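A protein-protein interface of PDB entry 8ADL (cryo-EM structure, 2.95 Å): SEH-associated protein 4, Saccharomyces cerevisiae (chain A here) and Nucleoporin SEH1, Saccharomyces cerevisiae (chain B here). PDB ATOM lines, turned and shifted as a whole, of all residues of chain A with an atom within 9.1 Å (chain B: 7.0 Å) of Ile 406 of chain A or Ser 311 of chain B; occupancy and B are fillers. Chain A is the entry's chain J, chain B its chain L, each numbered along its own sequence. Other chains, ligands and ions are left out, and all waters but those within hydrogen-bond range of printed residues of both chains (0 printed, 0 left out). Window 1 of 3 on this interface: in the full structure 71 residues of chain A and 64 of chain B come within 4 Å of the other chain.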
ATOM      1  N   CYS A 402      -3.461 -16.237  19.798  1.00  0.00           N
ATOM      2  CA  CYS A 402      -2.214 -16.154  19.048  1.00  0.00           C
ATOM      3  C   CYS A 402      -1.287 -15.115  19.669  1.00  0.00           C
ATOM      4  O   CYS A 402      -1.702 -13.987  19.951  1.00  0.00           O
ATOM      5  CB  CYS A 402      -2.495 -15.810  17.588  1.00  0.00           C
ATOM      6  SG  CYS A 402      -1.019 -15.724  16.549  1.00  0.00           S
ATOM      7  N   SER A 403      -0.028 -15.497  19.878  1.00  0.00           N
ATOM      8  CA  SER A 403       0.950 -14.612  20.498  1.00  0.00           C
ATOM      9  C   SER A 403       1.758 -13.811  19.490  1.00  0.00           C
ATOM     10  O   SER A 403       2.164 -12.683  19.793  1.00  0.00           O
ATOM     11  CB  SER A 403       1.907 -15.421  21.376  1.00  0.00           C
ATOM     12  OG  SER A 403       2.745 -16.248  20.587  1.00  0.00           O
ATOM     13  N   LYS A 404       2.006 -14.361  18.304  1.00  0.00           N
ATOM     14  CA  LYS A 404       2.778 -13.661  17.287  1.00  0.00           C
ATOM     15  C   LYS A 404       2.325 -14.107  15.908  1.00  0.00           C
ATOM     16  O   LYS A 404       2.243 -15.308  15.638  1.00  0.00           O
ATOM     17  CB  LYS A 404       4.281 -13.912  17.453  1.00  0.00           C
ATOM     18  CG  LYS A 404       5.140 -12.864  16.773  1.00  0.00           C
ATOM     19  CD  LYS A 404       6.539 -12.797  17.355  1.00  0.00           C
ATOM     20  CE  LYS A 404       7.198 -11.471  17.009  1.00  0.00           C
ATOM     21  NZ  LYS A 404       8.664 -11.480  17.258  1.00  0.00           N
ATOM     22  N   ALA A 405       2.033 -13.139  15.044  1.00  0.00           N
ATOM     23  CA  ALA A 405       1.672 -13.389  13.652  1.00  0.00           C
ATOM     24  C   ALA A 405       2.688 -12.663  12.777  1.00  0.00           C
ATOM     25  O   ALA A 405       2.466 -11.525  12.359  1.00  0.00           O
ATOM     26  CB  ALA A 405       0.248 -12.930  13.359  1.00  0.00           C
ATOM     27  N   ILE A 406       3.803 -13.328  12.501  1.00  0.00           N
ATOM     28  CA  ILE A 406       4.883 -12.757  11.704  1.00  0.00           C
ATOM     29  C   ILE A 406       4.657 -13.095  10.240  1.00  0.00           C
ATOM     30  O   ILE A 406       4.253 -14.211   9.896  1.00  0.00           O
ATOM     31  CB  ILE A 406       6.255 -13.268  12.181  1.00  0.00           C
ATOM     32  CG1 ILE A 406       6.200 -14.773  12.443  1.00  0.00           C
ATOM     33  CG2 ILE A 406       6.708 -12.511  13.416  1.00  0.00           C
ATOM     34  CD1 ILE A 406       7.548 -15.416  12.610  1.00  0.00           C
ATOM     35  N   LEU A 407       4.905 -12.123   9.374  1.00  0.00           N
ATOM     36  CA  LEU A 407       4.806 -12.328   7.942  1.00  0.00           C
ATOM     37  C   LEU A 407       6.189 -12.657   7.384  1.00  0.00           C
ATOM     38  O   LEU A 407       7.150 -12.878   8.127  1.00  0.00           O
ATOM     39  CB  LEU A 407       4.187 -11.096   7.282  1.00  0.00           C
ATOM     40  CG  LEU A 407       2.657 -11.063   7.292  1.00  0.00           C
ATOM     41  CD1 LEU A 407       2.153  -9.632   7.311  1.00  0.00           C
ATOM     42  CD2 LEU A 407       2.096 -11.819   6.103  1.00  0.00           C
ATOM     43  N   ASN A 408       6.299 -12.689   6.059  1.00  0.00           N
ATOM     44  CA  ASN A 408       7.507 -13.136   5.386  1.00  0.00           C
ATOM     45  C   ASN A 408       7.727 -12.275   4.150  1.00  0.00           C
ATOM     46  O   ASN A 408       6.910 -11.413   3.813  1.00  0.00           O
ATOM     47  CB  ASN A 408       7.411 -14.619   5.016  1.00  0.00           C
ATOM     48  CG  ASN A 408       8.753 -15.309   5.027  1.00  0.00           C
ATOM     49  OD1 ASN A 408       9.732 -14.768   5.537  1.00  0.00           O
ATOM     50  ND2 ASN A 408       8.808 -16.509   4.462  1.00  0.00           N
ATOM     51  N   ASN A 409       8.848 -12.511   3.468  1.00  0.00           N
ATOM     52  CA  ASN A 409       9.051 -11.933   2.148  1.00  0.00           C
ATOM     53  C   ASN A 409       8.333 -12.715   1.057  1.00  0.00           C
ATOM     54  O   ASN A 409       8.238 -12.228  -0.074  1.00  0.00           O
ATOM     55  CB  ASN A 409      10.544 -11.853   1.827  1.00  0.00           C
ATOM     56  CG  ASN A 409      11.267 -13.153   2.099  1.00  0.00           C
ATOM     57  OD1 ASN A 409      11.025 -13.813   3.108  1.00  0.00           O
ATOM     58  ND2 ASN A 409      12.165 -13.530   1.196  1.00  0.00           N
ATOM     59  N   ASN A 411       5.133 -13.721   1.601  1.00  0.00           N
ATOM     60  CA  ASN A 411       3.752 -13.587   2.082  1.00  0.00           C
ATOM     61  C   ASN A 411       3.287 -14.849   2.810  1.00  0.00           C
ATOM     62  O   ASN A 411       2.193 -15.365   2.576  1.00  0.00           O
ATOM     63  CB  ASN A 411       2.792 -13.220   0.945  1.00  0.00           C
ATOM     64  CG  ASN A 411       2.516 -11.735   0.874  1.00  0.00           C
ATOM     65  OD1 ASN A 411       2.326 -11.082   1.895  1.00  0.00           O
ATOM     66  ND2 ASN A 411       2.494 -11.196  -0.338  1.00  0.00           N
ATOM     67  N   SER A 412       4.139 -15.344   3.701  1.00  0.00           N
ATOM     68  CA  SER A 412       3.847 -16.519   4.512  1.00  0.00           C
ATOM     69  C   SER A 412       3.626 -16.090   5.954  1.00  0.00           C
ATOM     70  O   SER A 412       4.459 -15.383   6.532  1.00  0.00           O
ATOM     71  CB  SER A 412       4.986 -17.537   4.431  1.00  0.00           C
ATOM     72  OG  SER A 412       5.038 -18.142   3.151  1.00  0.00           O
ATOM     73  N   LEU A 413       2.507 -16.515   6.531  1.00  0.00           N
ATOM     74  CA  LEU A 413       2.121 -16.128   7.881  1.00  0.00           C
ATOM     75  C   LEU A 413       2.436 -17.261   8.846  1.00  0.00           C
ATOM     76  O   LEU A 413       2.128 -18.424   8.567  1.00  0.00           O
ATOM     77  CB  LEU A 413       0.634 -15.776   7.945  1.00  0.00           C
ATOM     78  CG  LEU A 413       0.167 -15.063   9.213  1.00  0.00           C
ATOM     79  CD1 LEU A 413       0.954 -13.781   9.429  1.00  0.00           C
ATOM     80  CD2 LEU A 413      -1.318 -14.774   9.146  1.00  0.00           C
ATOM     81  N   LEU A 414       3.049 -16.919   9.975  1.00  0.00           N
ATOM     82  CA  LEU A 414       3.442 -17.884  10.995  1.00  0.00           C
ATOM     83  C   LEU A 414       2.795 -17.488  12.313  1.00  0.00           C
ATOM     84  O   LEU A 414       2.988 -16.365  12.790  1.00  0.00           O
ATOM     85  CB  LEU A 414       4.964 -17.946  11.126  1.00  0.00           C
ATOM     86  CG  LEU A 414       5.595 -19.247  11.613  1.00  0.00           C
ATOM     87  CD1 LEU A 414       5.089 -20.432  10.824  1.00  0.00           C
ATOM     88  CD2 LEU A 414       7.100 -19.158  11.510  1.00  0.00           C
ATOM     89  N   LEU A 415       2.035 -18.408  12.900  1.00  0.00           N
ATOM     90  CA  LEU A 415       1.207 -18.128  14.065  1.00  0.00           C
ATOM     91  C   LEU A 415       1.709 -18.931  15.255  1.00  0.00           C
ATOM     92  O   LEU A 415       1.905 -20.145  15.150  1.00  0.00           O
ATOM     93  CB  LEU A 415      -0.263 -18.464  13.792  1.00  0.00           C
ATOM     94  CG  LEU A 415      -1.076 -17.574  12.849  1.00  0.00           C
ATOM     95  CD1 LEU A 415      -0.922 -17.997  11.397  1.00  0.00           C
ATOM     96  CD2 LEU A 415      -2.537 -17.604  13.253  1.00  0.00           C
ATOM     97  N   SER A 416       1.890 -18.259  16.389  1.00  0.00           N
ATOM     98  CA  SER A 416       2.335 -18.891  17.620  1.00  0.00           C
ATOM     99  C   SER A 416       1.296 -18.661  18.706  1.00  0.00           C
ATOM    100  O   SER A 416       0.796 -17.543  18.868  1.00  0.00           O
ATOM    101  CB  SER A 416       3.690 -18.342  18.067  1.00  0.00           C
ATOM    102  OG  SER A 416       4.608 -18.335  16.991  1.00  0.00           O
ATOM    103  N   ILE A 423       3.194 -24.689  15.973  1.00  0.00           N
ATOM    104  CA  ILE A 423       3.232 -23.421  15.258  1.00  0.00           C
ATOM    105  C   ILE A 423       2.475 -23.587  13.948  1.00  0.00           C
ATOM    106  O   ILE A 423       2.753 -24.515  13.180  1.00  0.00           O
ATOM    107  CB  ILE A 423       4.682 -22.967  15.003  1.00  0.00           C
ATOM    108  CG1 ILE A 423       5.463 -22.892  16.316  1.00  0.00           C
ATOM    109  CG2 ILE A 423       4.710 -21.626  14.321  1.00  0.00           C
ATOM    110  CD1 ILE A 423       4.884 -21.916  17.318  1.00  0.00           C
ATOM    111  N   ASP A 424       1.520 -22.695  13.697  1.00  0.00           N
ATOM    112  CA  ASP A 424       0.697 -22.751  12.496  1.00  0.00           C
ATOM    113  C   ASP A 424       1.297 -21.893  11.389  1.00  0.00           C
ATOM    114  O   ASP A 424       1.873 -20.834  11.651  1.00  0.00           O
ATOM    115  CB  ASP A 424      -0.727 -22.287  12.801  1.00  0.00           C
ATOM    116  CG  ASP A 424      -1.391 -23.115  13.882  1.00  0.00           C
ATOM    117  OD1 ASP A 424      -0.860 -24.196  14.213  1.00  0.00           O
ATOM    118  OD2 ASP A 424      -2.442 -22.685  14.402  1.00  0.00           O
ATOM    119  N   GLU A 425       1.150 -22.356  10.149  1.00  0.00           N
ATOM    120  CA  GLU A 425       1.731 -21.698   8.986  1.00  0.00           C
ATOM    121  C   GLU A 425       0.681 -21.589   7.890  1.00  0.00           C
ATOM    122  O   GLU A 425       0.022 -22.579   7.558  1.00  0.00           O
ATOM    123  CB  GLU A 425       2.957 -22.469   8.479  1.00  0.00           C
ATOM    124  CG  GLU A 425       3.328 -22.198   7.028  1.00  0.00           C
ATOM    125  CD  GLU A 425       3.913 -20.815   6.810  1.00  0.00           C
ATOM    126  OE1 GLU A 425       4.773 -20.394   7.607  1.00  0.00           O
ATOM    127  OE2 GLU A 425       3.510 -20.139   5.843  1.00  0.00           O
ATOM    128  N   ILE A 426       0.528 -20.390   7.333  1.00  0.00           N
ATOM    129  CA  ILE A 426      -0.351 -20.140   6.196  1.00  0.00           C
ATOM    130  C   ILE A 426       0.542 -19.756   5.024  1.00  0.00           C
ATOM    131  O   ILE A 426       0.971 -18.602   4.907  1.00  0.00           O
ATOM    132  CB  ILE A 426      -1.384 -19.048   6.495  1.00  0.00           C
ATOM    133  CG1 ILE A 426      -2.093 -19.332   7.819  1.00  0.00           C
ATOM    134  CG2 ILE A 426      -2.388 -18.942   5.358  1.00  0.00           C
ATOM    135  CD1 ILE A 426      -3.156 -18.316   8.175  1.00  0.00           C
ATOM    136  N   LEU A 503      -3.190 -13.202   0.618  1.00  0.00           N
ATOM    137  CA  LEU A 503      -1.733 -13.231   0.531  1.00  0.00           C
ATOM    138  C   LEU A 503      -1.259 -13.516  -0.890  1.00  0.00           C
ATOM    139  O   LEU A 503      -0.169 -13.080  -1.276  1.00  0.00           O
ATOM    140  CB  LEU A 503      -1.167 -14.263   1.505  1.00  0.00           C
ATOM    141  CG  LEU A 503      -1.348 -13.948   2.991  1.00  0.00           C
ATOM    142  CD1 LEU A 503      -1.115 -15.188   3.835  1.00  0.00           C
ATOM    143  CD2 LEU A 503      -0.423 -12.825   3.420  1.00  0.00           C
ATOM    144  N   ASP B  14       9.121 -16.206  21.310  1.00  0.00           N
ATOM    145  CA  ASP B  14       9.427 -15.406  20.131  1.00  0.00           C
ATOM    146  C   ASP B  14       9.788 -16.310  18.962  1.00  0.00           C
ATOM    147  O   ASP B  14      10.666 -17.169  19.082  1.00  0.00           O
ATOM    148  CB  ASP B  14      10.571 -14.427  20.409  1.00  0.00           C
ATOM    149  CG  ASP B  14      10.566 -13.244  19.463  1.00  0.00           C
ATOM    150  OD1 ASP B  14       9.671 -13.180  18.596  1.00  0.00           O
ATOM    151  OD2 ASP B  14      11.456 -12.378  19.585  1.00  0.00           O
ATOM    152  N   VAL B  15       9.106 -16.112  17.837  1.00  0.00           N
ATOM    153  CA  VAL B  15       9.450 -16.741  16.568  1.00  0.00           C
ATOM    154  C   VAL B  15       9.792 -15.634  15.583  1.00  0.00           C
ATOM    155  O   VAL B  15       9.023 -14.680  15.428  1.00  0.00           O
ATOM    156  CB  VAL B  15       8.304 -17.619  16.036  1.00  0.00           C
ATOM    157  CG1 VAL B  15       8.726 -18.318  14.758  1.00  0.00           C
ATOM    158  CG2 VAL B  15       7.892 -18.636  17.080  1.00  0.00           C
ATOM    159  N   VAL B  16      10.959 -15.738  14.947  1.00  0.00           N
ATOM    160  CA  VAL B  16      11.433 -14.737  13.997  1.00  0.00           C
ATOM    161  C   VAL B  16      11.927 -15.424  12.729  1.00  0.00           C
ATOM    162  O   VAL B  16      12.539 -16.497  12.784  1.00  0.00           O
ATOM    163  CB  VAL B  16      12.538 -13.834  14.599  1.00  0.00           C
ATOM    164  CG1 VAL B  16      11.968 -12.936  15.684  1.00  0.00           C
ATOM    165  CG2 VAL B  16      13.677 -14.666  15.168  1.00  0.00           C
ATOM    166  N   TYR B  17      11.621 -14.819  11.584  1.00  0.00           N
ATOM    167  CA  TYR B  17      12.194 -15.228  10.312  1.00  0.00           C
ATOM    168  C   TYR B  17      13.585 -14.623  10.143  1.00  0.00           C
ATOM    169  O   TYR B  17      13.993 -13.716  10.872  1.00  0.00           O
ATOM    170  CB  TYR B  17      11.306 -14.785   9.149  1.00  0.00           C
ATOM    171  CG  TYR B  17      10.193 -15.735   8.772  1.00  0.00           C
ATOM    172  CD1 TYR B  17      10.426 -16.797   7.911  1.00  0.00           C
ATOM    173  CD2 TYR B  17       8.907 -15.554   9.258  1.00  0.00           C
ATOM    174  CE1 TYR B  17       9.409 -17.661   7.551  1.00  0.00           C
ATOM    175  CE2 TYR B  17       7.885 -16.414   8.909  1.00  0.00           C
ATOM    176  CZ  TYR B  17       8.143 -17.465   8.057  1.00  0.00           C
ATOM    177  OH  TYR B  17       7.127 -18.323   7.706  1.00  0.00           O
ATOM    178  N   VAL B  24      13.558 -20.191  10.354  1.00  0.00           N
ATOM    179  CA  VAL B  24      12.887 -19.614  11.511  1.00  0.00           C
ATOM    180  C   VAL B  24      13.613 -20.080  12.760  1.00  0.00           C
ATOM    181  O   VAL B  24      14.112 -21.209  12.824  1.00  0.00           O
ATOM    182  CB  VAL B  24      11.384 -19.965  11.580  1.00  0.00           C
ATOM    183  CG1 VAL B  24      10.651 -19.351  10.421  1.00  0.00           C
ATOM    184  CG2 VAL B  24      11.155 -21.459  11.599  1.00  0.00           C
ATOM    185  N   ALA B  25      13.711 -19.188  13.734  1.00  0.00           N
ATOM    186  CA  ALA B  25      14.308 -19.490  15.022  1.00  0.00           C
ATOM    187  C   ALA B  25      13.247 -19.273  16.086  1.00  0.00           C
ATOM    188  O   ALA B  25      12.609 -18.216  16.125  1.00  0.00           O
ATOM    189  CB  ALA B  25      15.537 -18.618  15.282  1.00  0.00           C
ATOM    190  N   SER B 217       3.552  -4.451  21.170  1.00  0.00           N
ATOM    191  CA  SER B 217       4.377  -4.663  19.991  1.00  0.00           C
ATOM    192  C   SER B 217       4.453  -3.389  19.159  1.00  0.00           C
ATOM    193  O   SER B 217       3.451  -2.695  18.981  1.00  0.00           O
ATOM    194  CB  SER B 217       3.833  -5.824  19.156  1.00  0.00           C
ATOM    195  OG  SER B 217       2.558  -5.506  18.636  1.00  0.00           O
ATOM    196  N   ILE B 218       5.652  -3.099  18.661  1.00  0.00           N
ATOM    197  CA  ILE B 218       5.919  -1.971  17.774  1.00  0.00           C
ATOM    198  C   ILE B 218       6.567  -2.519  16.512  1.00  0.00           C
ATOM    199  O   ILE B 218       7.531  -3.288  16.590  1.00  0.00           O
ATOM    200  CB  ILE B 218       6.830  -0.923  18.442  1.00  0.00           C
ATOM    201  CG1 ILE B 218       6.170  -0.344  19.694  1.00  0.00           C
ATOM    202  CG2 ILE B 218       7.216   0.178  17.458  1.00  0.00           C
ATOM    203  CD1 ILE B 218       5.152   0.739  19.411  1.00  0.00           C
ATOM    204  N   SER B 219       6.041  -2.127  15.353  1.00  0.00           N
ATOM    205  CA  SER B 219       6.582  -2.579  14.077  1.00  0.00           C
ATOM    206  C   SER B 219       6.664  -1.400  13.121  1.00  0.00           C
ATOM    207  O   SER B 219       5.643  -0.784  12.800  1.00  0.00           O
ATOM    208  CB  SER B 219       5.722  -3.696  13.480  1.00  0.00           C
ATOM    209  OG  SER B 219       6.397  -4.343  12.415  1.00  0.00           O
ATOM    210  N   ALA B 232       3.282   0.755  13.240  1.00  0.00           N
ATOM    211  CA  ALA B 232       2.138   0.039  13.780  1.00  0.00           C
ATOM    212  C   ALA B 232       2.363  -0.253  15.257  1.00  0.00           C
ATOM    213  O   ALA B 232       3.487  -0.539  15.680  1.00  0.00           O
ATOM    214  CB  ALA B 232       1.906  -1.262  13.018  1.00  0.00           C
ATOM    215  N   SER B 309       0.520  -8.855  19.218  1.00  0.00           N
ATOM    216  CA  SER B 309       1.578  -8.647  18.244  1.00  0.00           C
ATOM    217  C   SER B 309       1.023  -7.905  17.040  1.00  0.00           C
ATOM    218  O   SER B 309      -0.138  -8.080  16.664  1.00  0.00           O
ATOM    219  CB  SER B 309       2.197  -9.971  17.788  1.00  0.00           C
ATOM    220  OG  SER B 309       1.324 -10.657  16.909  1.00  0.00           O
ATOM    221  N   VAL B 310       1.865  -7.072  16.436  1.00  0.00           N
ATOM    222  CA  VAL B 310       1.570  -6.473  15.144  1.00  0.00           C
ATOM    223  C   VAL B 310       2.816  -6.602  14.274  1.00  0.00           C
ATOM    224  O   VAL B 310       3.945  -6.490  14.765  1.00  0.00           O
ATOM    225  CB  VAL B 310       1.092  -5.004  15.270  1.00  0.00           C
ATOM    226  CG1 VAL B 310       2.180  -4.063  15.785  1.00  0.00           C
ATOM    227  CG2 VAL B 310       0.518  -4.517  13.966  1.00  0.00           C
ATOM    228  N   SER B 311       2.613  -6.913  12.997  1.00  0.00           N
ATOM    229  CA  SER B 311       3.728  -7.149  12.095  1.00  0.00           C
ATOM    230  C   SER B 311       3.350  -6.679  10.701  1.00  0.00           C
ATOM    231  O   SER B 311       2.171  -6.568  10.358  1.00  0.00           O
ATOM    232  CB  SER B 311       4.129  -8.628  12.069  1.00  0.00           C
ATOM    233  OG  SER B 311       3.204  -9.390  11.316  1.00  0.00           O
ATOM    234  N   TRP B 312       4.371  -6.405   9.900  1.00  0.00           N
ATOM    235  CA  TRP B 312       4.210  -5.900   8.547  1.00  0.00           C
ATOM    236  C   TRP B 312       4.659  -6.944   7.536  1.00  0.00           C
ATOM    237  O   TRP B 312       5.234  -7.980   7.878  1.00  0.00           O
ATOM    238  CB  TRP B 312       5.007  -4.609   8.346  1.00  0.00           C
ATOM    239  CG  TRP B 312       4.416  -3.403   8.991  1.00  0.00           C
ATOM    240  CD1 TRP B 312       4.829  -2.807  10.142  1.00  0.00           C
ATOM    241  CD2 TRP B 312       3.322  -2.622   8.503  1.00  0.00           C
ATOM    242  NE1 TRP B 312       4.051  -1.709  10.412  1.00  0.00           N
ATOM    243  CE2 TRP B 312       3.117  -1.574   9.420  1.00  0.00           C
ATOM    244  CE3 TRP B 312       2.490  -2.712   7.385  1.00  0.00           C
ATOM    245  CZ2 TRP B 312       2.119  -0.621   9.252  1.00  0.00           C
ATOM    246  CZ3 TRP B 312       1.497  -1.767   7.220  1.00  0.00           C
ATOM    247  CH2 TRP B 312       1.321  -0.735   8.148  1.00  0.00           C
ATOM    248  N   ASN B 313       4.384  -6.648   6.274  1.00  0.00           N
ATOM    249  CA  ASN B 313       4.807  -7.484   5.164  1.00  0.00           C
ATOM    250  C   ASN B 313       6.199  -7.036   4.722  1.00  0.00           C
ATOM    251  O   ASN B 313       6.856  -6.230   5.387  1.00  0.00           O
ATOM    252  CB  ASN B 313       3.777  -7.409   4.039  1.00  0.00           C
ATOM    253  CG  ASN B 313       3.736  -8.668   3.205  1.00  0.00           C
ATOM    254  OD1 ASN B 313       4.408  -9.651   3.512  1.00  0.00           O
ATOM    255  ND2 ASN B 313       2.940  -8.648   2.143  1.00  0.00           N
ATOM    256  N   ILE B 318       0.474  -5.256   4.106  1.00  0.00           N
ATOM    257  CA  ILE B 318      -0.386  -6.111   4.914  1.00  0.00           C
ATOM    258  C   ILE B 318       0.043  -5.974   6.367  1.00  0.00           C
ATOM    259  O   ILE B 318       1.223  -6.155   6.690  1.00  0.00           O
ATOM    260  CB  ILE B 318      -0.327  -7.580   4.453  1.00  0.00           C
ATOM    261  CG1 ILE B 318      -1.045  -7.745   3.111  1.00  0.00           C
ATOM    262  CG2 ILE B 318      -0.940  -8.503   5.498  1.00  0.00           C
ATOM    263  CD1 ILE B 318      -1.215  -9.184   2.674  1.00  0.00           C
ATOM    264  N   LEU B 319      -0.910  -5.652   7.236  1.00  0.00           N
ATOM    265  CA  LEU B 319      -0.687  -5.549   8.672  1.00  0.00           C
ATOM    266  C   LEU B 319      -1.374  -6.723   9.355  1.00  0.00           C
ATOM    267  O   LEU B 319      -2.599  -6.852   9.284  1.00  0.00           O
ATOM    268  CB  LEU B 319      -1.230  -4.220   9.197  1.00  0.00           C
ATOM    269  CG  LEU B 319      -0.991  -3.784  10.640  1.00  0.00           C
ATOM    270  CD1 LEU B 319      -0.736  -2.301  10.672  1.00  0.00           C
ATOM    271  CD2 LEU B 319      -2.187  -4.103  11.511  1.00  0.00           C
ATOM    272  N   SER B 320      -0.591  -7.563  10.025  1.00  0.00           N
ATOM    273  CA  SER B 320      -1.118  -8.718  10.742  1.00  0.00           C
ATOM    274  C   SER B 320      -1.144  -8.416  12.236  1.00  0.00           C
ATOM    275  O   SER B 320      -0.107  -8.098  12.825  1.00  0.00           O
ATOM    276  CB  SER B 320      -0.277  -9.963  10.459  1.00  0.00           C
ATOM    277  OG  SER B 320       0.895  -9.977  11.253  1.00  0.00           O
ATOM    278  N   SER B 321      -2.324  -8.523  12.843  1.00  0.00           N
ATOM    279  CA  SER B 321      -2.511  -8.239  14.259  1.00  0.00           C
ATOM    280  C   SER B 321      -3.194  -9.421  14.931  1.00  0.00           C
ATOM    281  O   SER B 321      -4.124 -10.008  14.373  1.00  0.00           O
ATOM    282  CB  SER B 321      -3.339  -6.969  14.466  1.00  0.00           C
ATOM    283  OG  SER B 321      -4.651  -7.131  13.958  1.00  0.00           O
ATOM    284  N   ALA B 322      -2.732  -9.761  16.132  1.00  0.00           N
ATOM    285  CA  ALA B 322      -3.275 -10.866  16.914  1.00  0.00           C
ATOM    286  C   ALA B 322      -3.826 -10.343  18.232  1.00  0.00           C
ATOM    287  O   ALA B 322      -3.146  -9.586  18.933  1.00  0.00           O
ATOM    288  CB  ALA B 322      -2.207 -11.932  17.173  1.00  0.00           C
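The side-chain hydroxyl (OG) of Ser 309 of chain B lies within hydrogen-bond range of the backbone NH (N) of Ala 405 of chain A.
The side-chain amide nitrogen of Asn 313 of chain B is in hydrogen-bond range of the side-chain amide oxygen of Asn 411 of chain A (2.5 Å).
The backbone carbonyl oxygen (O) of Ala 405 of chain A lies within hydrogen-bond range of the side-chain hydroxyl (OG) of Ser 311 of chain B (2.5 Å).
The backbone carbonyl oxygen (O) of Asn 408 of chain A lies close to the side-chain amide oxygen (OD1) of Asn 313 of chain B.
The side-chain hydroxyl (OH) of Tyr 17 of chain B sits at hydrogen-bond distance from the side-chain carboxylate (OE1) of Glu 425 of chain A (3.1 Å).
The side-chain hydroxyl (OG) of Ser 320 of chain B sits at hydrogen-bond distance from the backbone carbonyl oxygen (O) of Ala 405 of chain A.
The side-chain amino group of Lys 404 of chain A is in salt-bridge range of the side-chain carboxylate of Asp 14 of chain B.
O of Ser 416 of chain A is in hydrogen-bond range of N of Ser 403 of chain A.
The backbone NH of Ala 322 of chain B is in hydrogen-bond range of the backbone carbonyl oxygen of Ser 309 of chain B (3.1 Å).
The indole nitrogen (NE1) of Trp 312 of chain B is in hydrogen-bond range of the backbone carbonyl oxygen (O) of Ser 219 of chain B (3.0 Å).
The backbone carbonyl oxygen (O) of Ile 318 of chain B sits at hydrogen-bond distance from the backbone NH (N) of Asn 313 of chain B, 3.2 Å away.
The backbone carbonyl oxygen of Ile 406 of chain A is in hydrogen-bond range of the backbone NH of Leu 414 of chain A (3.0 Å).
The backbone NH (N) of Ser 320 of chain B lies within hydrogen-bond range of the backbone carbonyl oxygen (O) of Ser 311 of chain B, 3.0 Å away.
Val 15 of chain B touches Lys 404 of chain A (O to CD, 3.7 Å).
NZ of Lys 404 of chain A touches CG1 of Val 16 of chain B, 3.9 Å away.
Ser 309 of chain B touches Lys 404 of chain A.
CD2 of Tyr 17 of chain B touches CD1 of Ile 406 of chain A, at 3.6 Å.
CA of Ile 406 of chain A touches OG of Ser 311 of chain B, at 3.8 Å.
Tyr 17 of chain B touches Leu 407 of chain A (CD2 to O, 3.4 Å).
Leu 407 of chain A touches Ser 311 of chain B (N to OG, 3.8 Å).
Leu 407 of chain A touches Trp 312 of chain B.
Ile 318 of chain B touches Leu 407 of chain A.
Val 15 of chain B touches Leu 414 of chain A (CG1 to CD2, 3.7 Å).
Of the printed residues of chain B, Ser 403 of chain A touches Ser 309.
Of the printed residues of chain B, Ala 405 of chain A touches Ser 309, Ser 311 and Ser 320.
Of the printed residues of chain B, Leu 414 of chain A touches Val 15, Tyr 17 and Val 24.
Val 310 of chain B touches none of the printed residues of chain A.
Of chain A, only Ala 405 (2.5 Å), Ile 406 (3.8 Å) and Leu 407 (3.8 Å) come within 4 Å of Ser 311 of chain B.
The nearest residue of chain A that does not touch Ser 311 of chain B is Leu 413 of chain A (5.3 Å).
Printed residues of chain A that touch a printed residue of chain B: Cys 402, Ser 403, Lys 404, Ala 405, Ile 406, Leu 407, Asn 408, Asn 411, Ser 412, Leu 414, Ser 416, Glu 425 and Leu 503.
Hydrophobic or aromatic side chains of chain A that line the printed part of chain B: Ala 405, Ile 406, Leu 407, Leu 414 and Leu 503.
Hydrophobic or aromatic side chains of chain B that line the printed part of chain A: Val 15, Val 16, Tyr 17, Val 24, Ile 318 and Ala 322.
Among the printed residues, 28 pairs touch across the chains.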
